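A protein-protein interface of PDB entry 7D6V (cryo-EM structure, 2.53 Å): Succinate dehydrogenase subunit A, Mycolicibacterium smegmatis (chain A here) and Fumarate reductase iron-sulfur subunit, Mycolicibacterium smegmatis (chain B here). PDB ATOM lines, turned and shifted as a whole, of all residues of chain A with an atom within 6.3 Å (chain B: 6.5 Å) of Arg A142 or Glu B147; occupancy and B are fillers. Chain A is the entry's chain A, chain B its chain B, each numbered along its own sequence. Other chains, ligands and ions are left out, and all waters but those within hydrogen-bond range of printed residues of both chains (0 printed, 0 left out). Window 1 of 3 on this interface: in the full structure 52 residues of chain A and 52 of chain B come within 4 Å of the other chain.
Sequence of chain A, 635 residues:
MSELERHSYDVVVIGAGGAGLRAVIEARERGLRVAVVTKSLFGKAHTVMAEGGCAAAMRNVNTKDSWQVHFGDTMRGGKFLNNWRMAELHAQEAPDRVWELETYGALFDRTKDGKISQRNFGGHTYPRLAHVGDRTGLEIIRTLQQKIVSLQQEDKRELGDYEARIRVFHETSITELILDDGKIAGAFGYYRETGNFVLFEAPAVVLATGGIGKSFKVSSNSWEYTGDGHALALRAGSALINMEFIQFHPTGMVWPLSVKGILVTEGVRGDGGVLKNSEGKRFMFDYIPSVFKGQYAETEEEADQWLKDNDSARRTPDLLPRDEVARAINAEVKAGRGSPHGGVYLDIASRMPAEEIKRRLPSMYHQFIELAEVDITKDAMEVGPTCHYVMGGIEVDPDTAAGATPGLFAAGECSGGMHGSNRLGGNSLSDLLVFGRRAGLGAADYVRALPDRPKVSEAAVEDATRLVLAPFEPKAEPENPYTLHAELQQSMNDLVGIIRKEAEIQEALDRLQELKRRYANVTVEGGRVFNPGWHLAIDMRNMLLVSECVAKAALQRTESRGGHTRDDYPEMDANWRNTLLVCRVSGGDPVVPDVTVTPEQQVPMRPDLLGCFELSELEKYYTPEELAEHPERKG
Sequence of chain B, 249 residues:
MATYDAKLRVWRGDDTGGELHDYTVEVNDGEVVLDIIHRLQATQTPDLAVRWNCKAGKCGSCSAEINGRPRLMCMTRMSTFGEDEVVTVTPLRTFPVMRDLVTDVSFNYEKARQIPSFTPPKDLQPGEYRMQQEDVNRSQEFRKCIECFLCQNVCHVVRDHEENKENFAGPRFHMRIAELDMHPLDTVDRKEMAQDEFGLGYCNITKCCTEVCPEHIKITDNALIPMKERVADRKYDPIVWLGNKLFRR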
ATOM      1  N   LEU A  41     -17.978 -28.450   2.095  1.00  0.00           N
ATOM      2  CA  LEU A  41     -18.670 -27.933   0.926  1.00  0.00           C
ATOM      3  C   LEU A  41     -18.607 -26.407   0.905  1.00  0.00           C
ATOM      4  O   LEU A  41     -18.358 -25.751   1.920  1.00  0.00           O
ATOM      5  CB  LEU A  41     -20.127 -28.399   0.910  1.00  0.00           C
ATOM      6  CG  LEU A  41     -20.401 -29.868   0.575  1.00  0.00           C
ATOM      7  CD1 LEU A  41     -21.880 -30.183   0.706  1.00  0.00           C
ATOM      8  CD2 LEU A  41     -19.915 -30.208  -0.811  1.00  0.00           C
ATOM      9  N   PHE A  42     -18.830 -25.843  -0.278  1.00  0.00           N
ATOM     10  CA  PHE A  42     -18.756 -24.399  -0.456  1.00  0.00           C
ATOM     11  C   PHE A  42     -19.854 -23.704   0.342  1.00  0.00           C
ATOM     12  O   PHE A  42     -21.040 -24.003   0.180  1.00  0.00           O
ATOM     13  CB  PHE A  42     -18.874 -24.055  -1.940  1.00  0.00           C
ATOM     14  CG  PHE A  42     -18.499 -22.642  -2.274  1.00  0.00           C
ATOM     15  CD1 PHE A  42     -17.575 -21.955  -1.510  1.00  0.00           C
ATOM     16  CD2 PHE A  42     -19.068 -22.001  -3.360  1.00  0.00           C
ATOM     17  CE1 PHE A  42     -17.231 -20.657  -1.821  1.00  0.00           C
ATOM     18  CE2 PHE A  42     -18.725 -20.707  -3.676  1.00  0.00           C
ATOM     19  CZ  PHE A  42     -17.807 -20.033  -2.904  1.00  0.00           C
ATOM     20  N   GLY A  43     -19.454 -22.768   1.200  1.00  0.00           N
ATOM     21  CA  GLY A  43     -20.407 -22.033   2.006  1.00  0.00           C
ATOM     22  C   GLY A  43     -20.818 -22.699   3.297  1.00  0.00           C
ATOM     23  O   GLY A  43     -21.823 -22.299   3.889  1.00  0.00           O
ATOM     24  N   LYS A  44     -20.075 -23.703   3.758  1.00  0.00           N
ATOM     25  CA  LYS A  44     -20.429 -24.456   4.956  1.00  0.00           C
ATOM     26  C   LYS A  44     -19.322 -24.416   6.004  1.00  0.00           C
ATOM     27  O   LYS A  44     -19.175 -25.348   6.794  1.00  0.00           O
ATOM     28  CB  LYS A  44     -20.772 -25.901   4.599  1.00  0.00           C
ATOM     29  CG  LYS A  44     -21.865 -26.034   3.562  1.00  0.00           C
ATOM     30  CD  LYS A  44     -22.560 -27.374   3.667  1.00  0.00           C
ATOM     31  CE  LYS A  44     -23.704 -27.475   2.683  1.00  0.00           C
ATOM     32  NZ  LYS A  44     -24.579 -26.281   2.737  1.00  0.00           N
ATOM     33  N   VAL A  48     -20.685 -19.978   9.600  1.00  0.00           N
ATOM     34  CA  VAL A  48     -22.144 -20.046   9.588  1.00  0.00           C
ATOM     35  C   VAL A  48     -22.723 -20.130  10.992  1.00  0.00           C
ATOM     36  O   VAL A  48     -23.892 -19.790  11.199  1.00  0.00           O
ATOM     37  CB  VAL A  48     -22.638 -21.248   8.751  1.00  0.00           C
ATOM     38  CG1 VAL A  48     -22.139 -21.158   7.331  1.00  0.00           C
ATOM     39  CG2 VAL A  48     -22.240 -22.567   9.392  1.00  0.00           C
ATOM     40  N   GLY A 137     -23.393 -14.631  11.013  1.00  0.00           N
ATOM     41  CA  GLY A 137     -22.357 -15.377  10.317  1.00  0.00           C
ATOM     42  C   GLY A 137     -22.859 -16.016   9.037  1.00  0.00           C
ATOM     43  O   GLY A 137     -22.164 -16.018   8.015  1.00  0.00           O
ATOM     44  N   LEU A 138     -24.075 -16.562   9.074  1.00  0.00           N
ATOM     45  CA  LEU A 138     -24.679 -17.118   7.870  1.00  0.00           C
ATOM     46  C   LEU A 138     -24.856 -16.050   6.801  1.00  0.00           C
ATOM     47  O   LEU A 138     -24.567 -16.289   5.623  1.00  0.00           O
ATOM     48  CB  LEU A 138     -26.022 -17.761   8.208  1.00  0.00           C
ATOM     49  CG  LEU A 138     -26.836 -18.278   7.023  1.00  0.00           C
ATOM     50  CD1 LEU A 138     -26.198 -19.526   6.446  1.00  0.00           C
ATOM     51  CD2 LEU A 138     -28.270 -18.545   7.433  1.00  0.00           C
ATOM     52  N   GLU A 139     -25.320 -14.863   7.194  1.00  0.00           N
ATOM     53  CA  GLU A 139     -25.483 -13.775   6.236  1.00  0.00           C
ATOM     54  C   GLU A 139     -24.148 -13.384   5.618  1.00  0.00           C
ATOM     55  O   GLU A 139     -24.050 -13.198   4.399  1.00  0.00           O
ATOM     56  CB  GLU A 139     -26.132 -12.574   6.923  1.00  0.00           C
ATOM     57  CG  GLU A 139     -26.353 -11.369   6.027  1.00  0.00           C
ATOM     58  CD  GLU A 139     -27.531 -11.540   5.091  1.00  0.00           C
ATOM     59  OE1 GLU A 139     -27.352 -11.353   3.873  1.00  0.00           O
ATOM     60  OE2 GLU A 139     -28.636 -11.861   5.572  1.00  0.00           O
ATOM     61  N   ILE A 140     -23.104 -13.282   6.441  1.00  0.00           N
ATOM     62  CA  ILE A 140     -21.788 -12.889   5.944  1.00  0.00           C
ATOM     63  C   ILE A 140     -21.273 -13.907   4.935  1.00  0.00           C
ATOM     64  O   ILE A 140     -20.824 -13.552   3.836  1.00  0.00           O
ATOM     65  CB  ILE A 140     -20.807 -12.719   7.117  1.00  0.00           C
ATOM     66  CG1 ILE A 140     -21.156 -11.475   7.925  1.00  0.00           C
ATOM     67  CG2 ILE A 140     -19.380 -12.635   6.615  1.00  0.00           C
ATOM     68  CD1 ILE A 140     -20.555 -11.482   9.296  1.00  0.00           C
ATOM     69  N   ILE A 141     -21.332 -15.192   5.291  1.00  0.00           N
ATOM     70  CA  ILE A 141     -20.753 -16.213   4.424  1.00  0.00           C
ATOM     71  C   ILE A 141     -21.578 -16.375   3.148  1.00  0.00           C
ATOM     72  O   ILE A 141     -21.020 -16.570   2.061  1.00  0.00           O
ATOM     73  CB  ILE A 141     -20.578 -17.538   5.191  1.00  0.00           C
ATOM     74  CG1 ILE A 141     -19.641 -18.477   4.429  1.00  0.00           C
ATOM     75  CG2 ILE A 141     -21.911 -18.199   5.472  1.00  0.00           C
ATOM     76  CD1 ILE A 141     -19.096 -19.604   5.268  1.00  0.00           C
ATOM     77  N   ARG A 142     -22.909 -16.272   3.248  1.00  0.00           N
ATOM     78  CA  ARG A 142     -23.746 -16.315   2.054  1.00  0.00           C
ATOM     79  C   ARG A 142     -23.419 -15.161   1.124  1.00  0.00           C
ATOM     80  O   ARG A 142     -23.303 -15.347  -0.093  1.00  0.00           O
ATOM     81  CB  ARG A 142     -25.222 -16.254   2.439  1.00  0.00           C
ATOM     82  CG  ARG A 142     -25.873 -17.583   2.705  1.00  0.00           C
ATOM     83  CD  ARG A 142     -25.958 -18.477   1.484  1.00  0.00           C
ATOM     84  NE  ARG A 142     -26.305 -19.826   1.914  1.00  0.00           N
ATOM     85  CZ  ARG A 142     -25.430 -20.689   2.413  1.00  0.00           C
ATOM     86  NH1 ARG A 142     -24.156 -20.352   2.522  1.00  0.00           N
ATOM     87  NH2 ARG A 142     -25.824 -21.889   2.798  1.00  0.00           N
ATOM     88  N   THR A 143     -23.275 -13.957   1.680  1.00  0.00           N
ATOM     89  CA  THR A 143     -22.979 -12.792   0.862  1.00  0.00           C
ATOM     90  C   THR A 143     -21.642 -12.946   0.154  1.00  0.00           C
ATOM     91  O   THR A 143     -21.528 -12.654  -1.041  1.00  0.00           O
ATOM     92  CB  THR A 143     -22.990 -11.537   1.732  1.00  0.00           C
ATOM     93  OG1 THR A 143     -24.167 -11.539   2.546  1.00  0.00           O
ATOM     94  CG2 THR A 143     -23.001 -10.302   0.878  1.00  0.00           C
ATOM     95  N   LEU A 144     -20.624 -13.423   0.870  1.00  0.00           N
ATOM     96  CA  LEU A 144     -19.313 -13.595   0.248  1.00  0.00           C
ATOM     97  C   LEU A 144     -19.344 -14.660  -0.845  1.00  0.00           C
ATOM     98  O   LEU A 144     -18.773 -14.464  -1.926  1.00  0.00           O
ATOM     99  CB  LEU A 144     -18.276 -13.937   1.313  1.00  0.00           C
ATOM    100  CG  LEU A 144     -17.958 -12.805   2.287  1.00  0.00           C
ATOM    101  CD1 LEU A 144     -17.076 -13.305   3.408  1.00  0.00           C
ATOM    102  CD2 LEU A 144     -17.300 -11.645   1.569  1.00  0.00           C
ATOM    103  N   GLN A 145     -20.011 -15.787  -0.588  1.00  0.00           N
ATOM    104  CA  GLN A 145     -20.092 -16.848  -1.590  1.00  0.00           C
ATOM    105  C   GLN A 145     -20.839 -16.383  -2.838  1.00  0.00           C
ATOM    106  O   GLN A 145     -20.419 -16.662  -3.970  1.00  0.00           O
ATOM    107  CB  GLN A 145     -20.759 -18.073  -0.968  1.00  0.00           C
ATOM    108  CG  GLN A 145     -21.366 -19.053  -1.941  1.00  0.00           C
ATOM    109  CD  GLN A 145     -22.272 -20.046  -1.251  1.00  0.00           C
ATOM    110  OE1 GLN A 145     -22.605 -19.884  -0.081  1.00  0.00           O
ATOM    111  NE2 GLN A 145     -22.674 -21.082  -1.970  1.00  0.00           N
ATOM    112  N   GLN A 146     -21.940 -15.653  -2.653  1.00  0.00           N
ATOM    113  CA  GLN A 146     -22.686 -15.152  -3.799  1.00  0.00           C
ATOM    114  C   GLN A 146     -21.915 -14.069  -4.541  1.00  0.00           C
ATOM    115  O   GLN A 146     -22.057 -13.937  -5.760  1.00  0.00           O
ATOM    116  CB  GLN A 146     -24.049 -14.643  -3.342  1.00  0.00           C
ATOM    117  CG  GLN A 146     -24.990 -15.760  -2.940  1.00  0.00           C
ATOM    118  CD  GLN A 146     -26.140 -15.281  -2.090  1.00  0.00           C
ATOM    119  OE1 GLN A 146     -26.183 -14.123  -1.681  1.00  0.00           O
ATOM    120  NE2 GLN A 146     -27.077 -16.172  -1.812  1.00  0.00           N
ATOM    121  N   LYS A 147     -21.085 -13.298  -3.837  1.00  0.00           N
ATOM    122  CA  LYS A 147     -20.212 -12.346  -4.514  1.00  0.00           C
ATOM    123  C   LYS A 147     -19.174 -13.064  -5.369  1.00  0.00           C
ATOM    124  O   LYS A 147     -18.858 -12.620  -6.478  1.00  0.00           O
ATOM    125  CB  LYS A 147     -19.543 -11.436  -3.486  1.00  0.00           C
ATOM    126  CG  LYS A 147     -18.543 -10.460  -4.065  1.00  0.00           C
ATOM    127  CD  LYS A 147     -19.200  -9.505  -5.036  1.00  0.00           C
ATOM    128  CE  LYS A 147     -18.200  -8.495  -5.556  1.00  0.00           C
ATOM    129  NZ  LYS A 147     -18.767  -7.663  -6.645  1.00  0.00           N
ATOM    130  N   CYS B  59     -25.848 -25.407   9.165  1.00  0.00           N
ATOM    131  CA  CYS B  59     -25.272 -25.686   7.858  1.00  0.00           C
ATOM    132  C   CYS B  59     -25.680 -26.313   6.535  1.00  0.00           C
ATOM    133  O   CYS B  59     -25.452 -25.741   5.463  1.00  0.00           O
ATOM    134  CB  CYS B  59     -23.739 -25.771   7.876  1.00  0.00           C
ATOM    135  SG  CYS B  59     -23.024 -27.329   8.448  1.00  0.00           S
ATOM    136  N   GLY B  60     -26.388 -27.699   6.741  1.00  0.00           N
ATOM    137  CA  GLY B  60     -26.706 -28.463   5.557  1.00  0.00           C
ATOM    138  C   GLY B  60     -25.787 -29.572   5.104  1.00  0.00           C
ATOM    139  O   GLY B  60     -25.971 -30.128   4.018  1.00  0.00           O
ATOM    140  N   SER B  61     -24.788 -29.900   5.920  1.00  0.00           N
ATOM    141  CA  SER B  61     -23.846 -30.944   5.538  1.00  0.00           C
ATOM    142  C   SER B  61     -24.438 -32.338   5.705  1.00  0.00           C
ATOM    143  O   SER B  61     -24.208 -33.215   4.867  1.00  0.00           O
ATOM    144  CB  SER B  61     -22.564 -30.813   6.356  1.00  0.00           C
ATOM    145  OG  SER B  61     -22.032 -29.508   6.260  1.00  0.00           O
ATOM    146  N   SER B  63     -27.356 -33.813   5.418  1.00  0.00           N
ATOM    147  CA  SER B  63     -28.627 -34.192   4.818  1.00  0.00           C
ATOM    148  C   SER B  63     -28.630 -35.674   4.464  1.00  0.00           C
ATOM    149  O   SER B  63     -27.701 -36.173   3.823  1.00  0.00           O
ATOM    150  CB  SER B  63     -28.893 -33.354   3.572  1.00  0.00           C
ATOM    151  OG  SER B  63     -28.900 -31.974   3.879  1.00  0.00           O
ATOM    152  N   TYR B 109     -24.679 -26.467  -7.130  1.00  0.00           N
ATOM    153  CA  TYR B 109     -23.666 -25.443  -7.346  1.00  0.00           C
ATOM    154  C   TYR B 109     -23.552 -25.052  -8.811  1.00  0.00           C
ATOM    155  O   TYR B 109     -23.110 -23.939  -9.110  1.00  0.00           O
ATOM    156  CB  TYR B 109     -22.322 -25.922  -6.802  1.00  0.00           C
ATOM    157  CG  TYR B 109     -22.325 -26.040  -5.298  1.00  0.00           C
ATOM    158  CD1 TYR B 109     -22.107 -24.930  -4.496  1.00  0.00           C
ATOM    159  CD2 TYR B 109     -22.574 -27.254  -4.679  1.00  0.00           C
ATOM    160  CE1 TYR B 109     -22.124 -25.029  -3.124  1.00  0.00           C
ATOM    161  CE2 TYR B 109     -22.593 -27.362  -3.308  1.00  0.00           C
ATOM    162  CZ  TYR B 109     -22.366 -26.247  -2.535  1.00  0.00           C
ATOM    163  OH  TYR B 109     -22.383 -26.350  -1.166  1.00  0.00           O
ATOM    164  N   ALA B 112     -26.383 -22.623  -9.197  1.00  0.00           N
ATOM    165  CA  ALA B 112     -26.179 -21.383  -8.458  1.00  0.00           C
ATOM    166  C   ALA B 112     -25.566 -20.287  -9.321  1.00  0.00           C
ATOM    167  O   ALA B 112     -25.827 -19.104  -9.081  1.00  0.00           O
ATOM    168  CB  ALA B 112     -25.301 -21.640  -7.235  1.00  0.00           C
ATOM    169  N   ARG B 143     -33.323 -15.399   3.112  1.00  0.00           N
ATOM    170  CA  ARG B 143     -31.902 -15.464   3.436  1.00  0.00           C
ATOM    171  C   ARG B 143     -31.603 -16.370   4.624  1.00  0.00           C
ATOM    172  O   ARG B 143     -30.431 -16.516   4.982  1.00  0.00           O
ATOM    173  CB  ARG B 143     -31.343 -14.069   3.711  1.00  0.00           C
ATOM    174  CG  ARG B 143     -31.529 -13.077   2.586  1.00  0.00           C
ATOM    175  CD  ARG B 143     -30.454 -13.215   1.540  1.00  0.00           C
ATOM    176  NE  ARG B 143     -29.177 -12.674   1.989  1.00  0.00           N
ATOM    177  CZ  ARG B 143     -28.042 -12.799   1.313  1.00  0.00           C
ATOM    178  NH1 ARG B 143     -28.030 -13.439   0.155  1.00  0.00           N
ATOM    179  NH2 ARG B 143     -26.921 -12.284   1.791  1.00  0.00           N
ATOM    180  N   CYS B 145     -31.952 -19.496   4.510  1.00  0.00           N
ATOM    181  CA  CYS B 145     -31.638 -20.800   3.926  1.00  0.00           C
ATOM    182  C   CYS B 145     -30.244 -21.430   4.034  1.00  0.00           C
ATOM    183  O   CYS B 145     -29.329 -21.050   3.303  1.00  0.00           O
ATOM    184  CB  CYS B 145     -32.072 -20.816   2.454  1.00  0.00           C
ATOM    185  SG  CYS B 145     -31.164 -21.989   1.420  1.00  0.00           S
ATOM    186  N   ILE B 146     -30.088 -22.395   4.941  1.00  0.00           N
ATOM    187  CA  ILE B 146     -28.842 -23.145   4.999  1.00  0.00           C
ATOM    188  C   ILE B 146     -28.874 -24.134   3.843  1.00  0.00           C
ATOM    189  O   ILE B 146     -29.818 -24.917   3.706  1.00  0.00           O
ATOM    190  CB  ILE B 146     -28.661 -23.845   6.358  1.00  0.00           C
ATOM    191  CG1 ILE B 146     -29.732 -24.910   6.603  1.00  0.00           C
ATOM    192  CG2 ILE B 146     -28.711 -22.831   7.482  1.00  0.00           C
ATOM    193  CD1 ILE B 146     -29.351 -25.936   7.629  1.00  0.00           C
ATOM    194  N   GLU B 147     -27.876 -24.074   2.974  1.00  0.00           N
ATOM    195  CA  GLU B 147     -28.005 -24.806   1.724  1.00  0.00           C
ATOM    196  C   GLU B 147     -27.863 -26.301   1.968  1.00  0.00           C
ATOM    197  O   GLU B 147     -26.838 -26.907   1.642  1.00  0.00           O
ATOM    198  CB  GLU B 147     -26.983 -24.299   0.709  1.00  0.00           C
ATOM    199  CG  GLU B 147     -27.371 -22.964   0.111  1.00  0.00           C
ATOM    200  CD  GLU B 147     -26.347 -22.439  -0.864  1.00  0.00           C
ATOM    201  OE1 GLU B 147     -25.158 -22.786  -0.724  1.00  0.00           O
ATOM    202  OE2 GLU B 147     -26.732 -21.678  -1.773  1.00  0.00           O
ATOM    203  N   CYS B 148     -28.917 -26.903   2.511  1.00  0.00           N
ATOM    204  CA  CYS B 148     -28.932 -28.336   2.775  1.00  0.00           C
ATOM    205  C   CYS B 148     -29.358 -29.089   1.518  1.00  0.00           C
ATOM    206  O   CYS B 148     -28.906 -30.207   1.268  1.00  0.00           O
ATOM    207  CB  CYS B 148     -29.877 -28.660   3.933  1.00  0.00           C
ATOM    208  SG  CYS B 148     -31.598 -28.919   3.442  1.00  0.00           S
ATOM    209  N   PHE B 149     -30.230 -28.466   0.731  1.00  0.00           N
ATOM    210  CA  PHE B 149     -30.723 -29.058  -0.510  1.00  0.00           C
ATOM    211  C   PHE B 149     -31.694 -30.204  -0.266  1.00  0.00           C
ATOM    212  O   PHE B 149     -31.889 -31.053  -1.140  1.00  0.00           O
ATOM    213  CB  PHE B 149     -29.561 -29.515  -1.397  1.00  0.00           C
ATOM    214  CG  PHE B 149     -28.536 -28.447  -1.642  1.00  0.00           C
ATOM    215  CD1 PHE B 149     -28.918 -27.189  -2.069  1.00  0.00           C
ATOM    216  CD2 PHE B 149     -27.194 -28.696  -1.428  1.00  0.00           C
ATOM    217  CE1 PHE B 149     -27.982 -26.204  -2.290  1.00  0.00           C
ATOM    218  CE2 PHE B 149     -26.254 -27.716  -1.648  1.00  0.00           C
ATOM    219  CZ  PHE B 149     -26.648 -26.467  -2.080  1.00  0.00           C
ATOM    220  N   LEU B 150     -32.324 -30.241   0.908  1.00  0.00           N
ATOM    221  CA  LEU B 150     -33.359 -31.238   1.156  1.00  0.00           C
ATOM    222  C   LEU B 150     -34.586 -30.972   0.294  1.00  0.00           C
ATOM    223  O   LEU B 150     -35.246 -31.910  -0.167  1.00  0.00           O
ATOM    224  CB  LEU B 150     -33.730 -31.255   2.637  1.00  0.00           C
ATOM    225  CG  LEU B 150     -32.712 -31.875   3.595  1.00  0.00           C
ATOM    226  CD1 LEU B 150     -33.115 -31.633   5.035  1.00  0.00           C
ATOM    227  CD2 LEU B 150     -32.544 -33.355   3.327  1.00  0.00           C
ATOM    228  N   ARG B 172     -34.964 -24.345  -4.189  1.00  0.00           N
ATOM    229  CA  ARG B 172     -34.014 -23.438  -3.553  1.00  0.00           C
ATOM    230  C   ARG B 172     -33.686 -22.261  -4.460  1.00  0.00           C
ATOM    231  O   ARG B 172     -33.636 -21.111  -4.010  1.00  0.00           O
ATOM    232  CB  ARG B 172     -32.741 -24.194  -3.168  1.00  0.00           C
ATOM    233  CG  ARG B 172     -31.787 -23.423  -2.268  1.00  0.00           C
ATOM    234  CD  ARG B 172     -30.681 -22.753  -3.070  1.00  0.00           C
ATOM    235  NE  ARG B 172     -29.877 -21.838  -2.268  1.00  0.00           N
ATOM    236  CZ  ARG B 172     -30.258 -20.618  -1.907  1.00  0.00           C
ATOM    237  NH1 ARG B 172     -29.453 -19.863  -1.175  1.00  0.00           N
ATOM    238  NH2 ARG B 172     -31.441 -20.152  -2.270  1.00  0.00           N
ATOM    239  N   PHE B 173     -33.500 -22.515  -5.747  1.00  0.00           N
ATOM    240  CA  PHE B 173     -33.043 -21.458  -6.634  1.00  0.00           C
ATOM    241  C   PHE B 173     -34.180 -20.618  -7.193  1.00  0.00           C
ATOM    242  O   PHE B 173     -33.974 -19.441  -7.497  1.00  0.00           O
ATOM    243  CB  PHE B 173     -32.189 -22.072  -7.736  1.00  0.00           C
ATOM    244  CG  PHE B 173     -30.928 -22.666  -7.209  1.00  0.00           C
ATOM    245  CD1 PHE B 173     -29.897 -21.850  -6.790  1.00  0.00           C
ATOM    246  CD2 PHE B 173     -30.802 -24.032  -7.056  1.00  0.00           C
ATOM    247  CE1 PHE B 173     -28.748 -22.385  -6.271  1.00  0.00           C
ATOM    248  CE2 PHE B 173     -29.652 -24.570  -6.536  1.00  0.00           C
ATOM    249  CZ  PHE B 173     -28.626 -23.746  -6.143  1.00  0.00           C
ATOM    250  N   ARG B 176     -34.384 -18.350  -4.460  1.00  0.00           N
ATOM    251  CA  ARG B 176     -33.329 -17.353  -4.624  1.00  0.00           C
ATOM    252  C   ARG B 176     -33.732 -16.278  -5.628  1.00  0.00           C
ATOM    253  O   ARG B 176     -33.457 -15.088  -5.425  1.00  0.00           O
ATOM    254  CB  ARG B 176     -32.034 -18.044  -5.052  1.00  0.00           C
ATOM    255  CG  ARG B 176     -30.957 -17.109  -5.551  1.00  0.00           C
ATOM    256  CD  ARG B 176     -29.975 -16.764  -4.454  1.00  0.00           C
ATOM    257  NE  ARG B 176     -28.845 -16.000  -4.968  1.00  0.00           N
ATOM    258  CZ  ARG B 176     -28.569 -14.750  -4.620  1.00  0.00           C
ATOM    259  NH1 ARG B 176     -29.340 -14.117  -3.750  1.00  0.00           N
ATOM    260  NH2 ARG B 176     -27.520 -14.135  -5.141  1.00  0.00           N
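Among the printed residues, merely in contact across the chains: Lys A44 with Ser B61 (3.4 Å), Gln A146 with Arg B176 (3.5 Å), Arg A142 with Cys B145 (3.5 Å), Leu A41 with Tyr B109 (3.7 Å), Lys A44 with Gly B60 (3.7 Å), Leu A138 with Arg B143 (3.8 Å), Val A48 with Cys B59 (3.8 Å) and Arg A142 with Ile B146 (3.9 Å).
Printed residues of chain B that touch a printed residue of chain A: Cys B59, Gly B60, Ser B61, Tyr B109, Arg B143, Cys B145, Ile B146, Glu B147 and Arg B176. Of the 16 printed residues of chain A, 10 touch a printed residue of chain B. Hydrophobic or aromatic side chains of chain A that line the printed part of chain B: Leu A41, Phe A42, Val A48 and Leu A138. Among the printed residues, 16 pairs touch across the chains.
The backbone carbonyl oxygen (O) of Phe A42 sits at hydrogen-bond distance from the side-chain hydroxyl (OH) of Tyr B109. The side-chain amino group of Lys A44 is in hydrogen-bond range of the backbone carbonyl oxygen of Cys B59 (2.9 Å). NZ of Lys A44 sits at hydrogen-bond distance from O of Glu B147, 2.6 Å away. OE1 of Glu A139 lies within salt-bridge range of NE of Arg B143 (2.9 Å). The side-chain carboxylate of Glu B147 is in salt-bridge range of the guanidinium group of Arg A142 (3.7 Å). NH2 of Arg B143 lies within hydrogen-bond range of OG1 of Thr A143 (3.0 Å). The side-chain carboxylate (OE1) of Glu B147 is in hydrogen-bond range of the side-chain amide nitrogen (NE2) of Gln A145 (3.3 Å). OE1 of Gln A146 sits at hydrogen-bond distance from NH1 of Arg B143.
Arg A142 touches just these residues of chain B: Cys B145 (3.5 Å), Ile B146 (3.9 Å) and Glu B147 (3.0 Å). Of the printed residues of chain A, Glu B147 touches Lys A44, Arg A142 and Gln A145. Printed residues of chain B within 4 Å of Phe A42: Tyr B109 (3.0 Å). Of the printed residues of chain B, Glu A139 touches Arg B143 (2.3 Å). Of the printed residues of chain A, Gly B60 touches Lys A44 (3.7 Å). The nearest residue of chain B that does not touch Arg A142 is Arg B143 (4.4 Å).
NH1 of Arg A142 lies within hydrogen-bond range of O of Gly A43 (3.3 Å). The backbone carbonyl oxygen (O) of Glu A139 is in hydrogen-bond range of the side-chain hydroxyl (OG1) of Thr A143, 2.5 Å away. The side-chain amide oxygen (OE1) of Gln A145 sits at hydrogen-bond distance from the guanidinium group (NH1) of Arg A142. The side-chain hydroxyl (OG) of Ser B61 sits close to the side-chain sulfur (SG) of Cys B59, 3.2 Å away. The side-chain sulfur (SG) of Cys B145 lies close to the guanidinium group (NH1) of Arg B172. The side-chain carboxylate (OE2) of Glu B147 lies within salt-bridge range of the guanidinium group (NE) of Arg B172 (3.2 Å).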
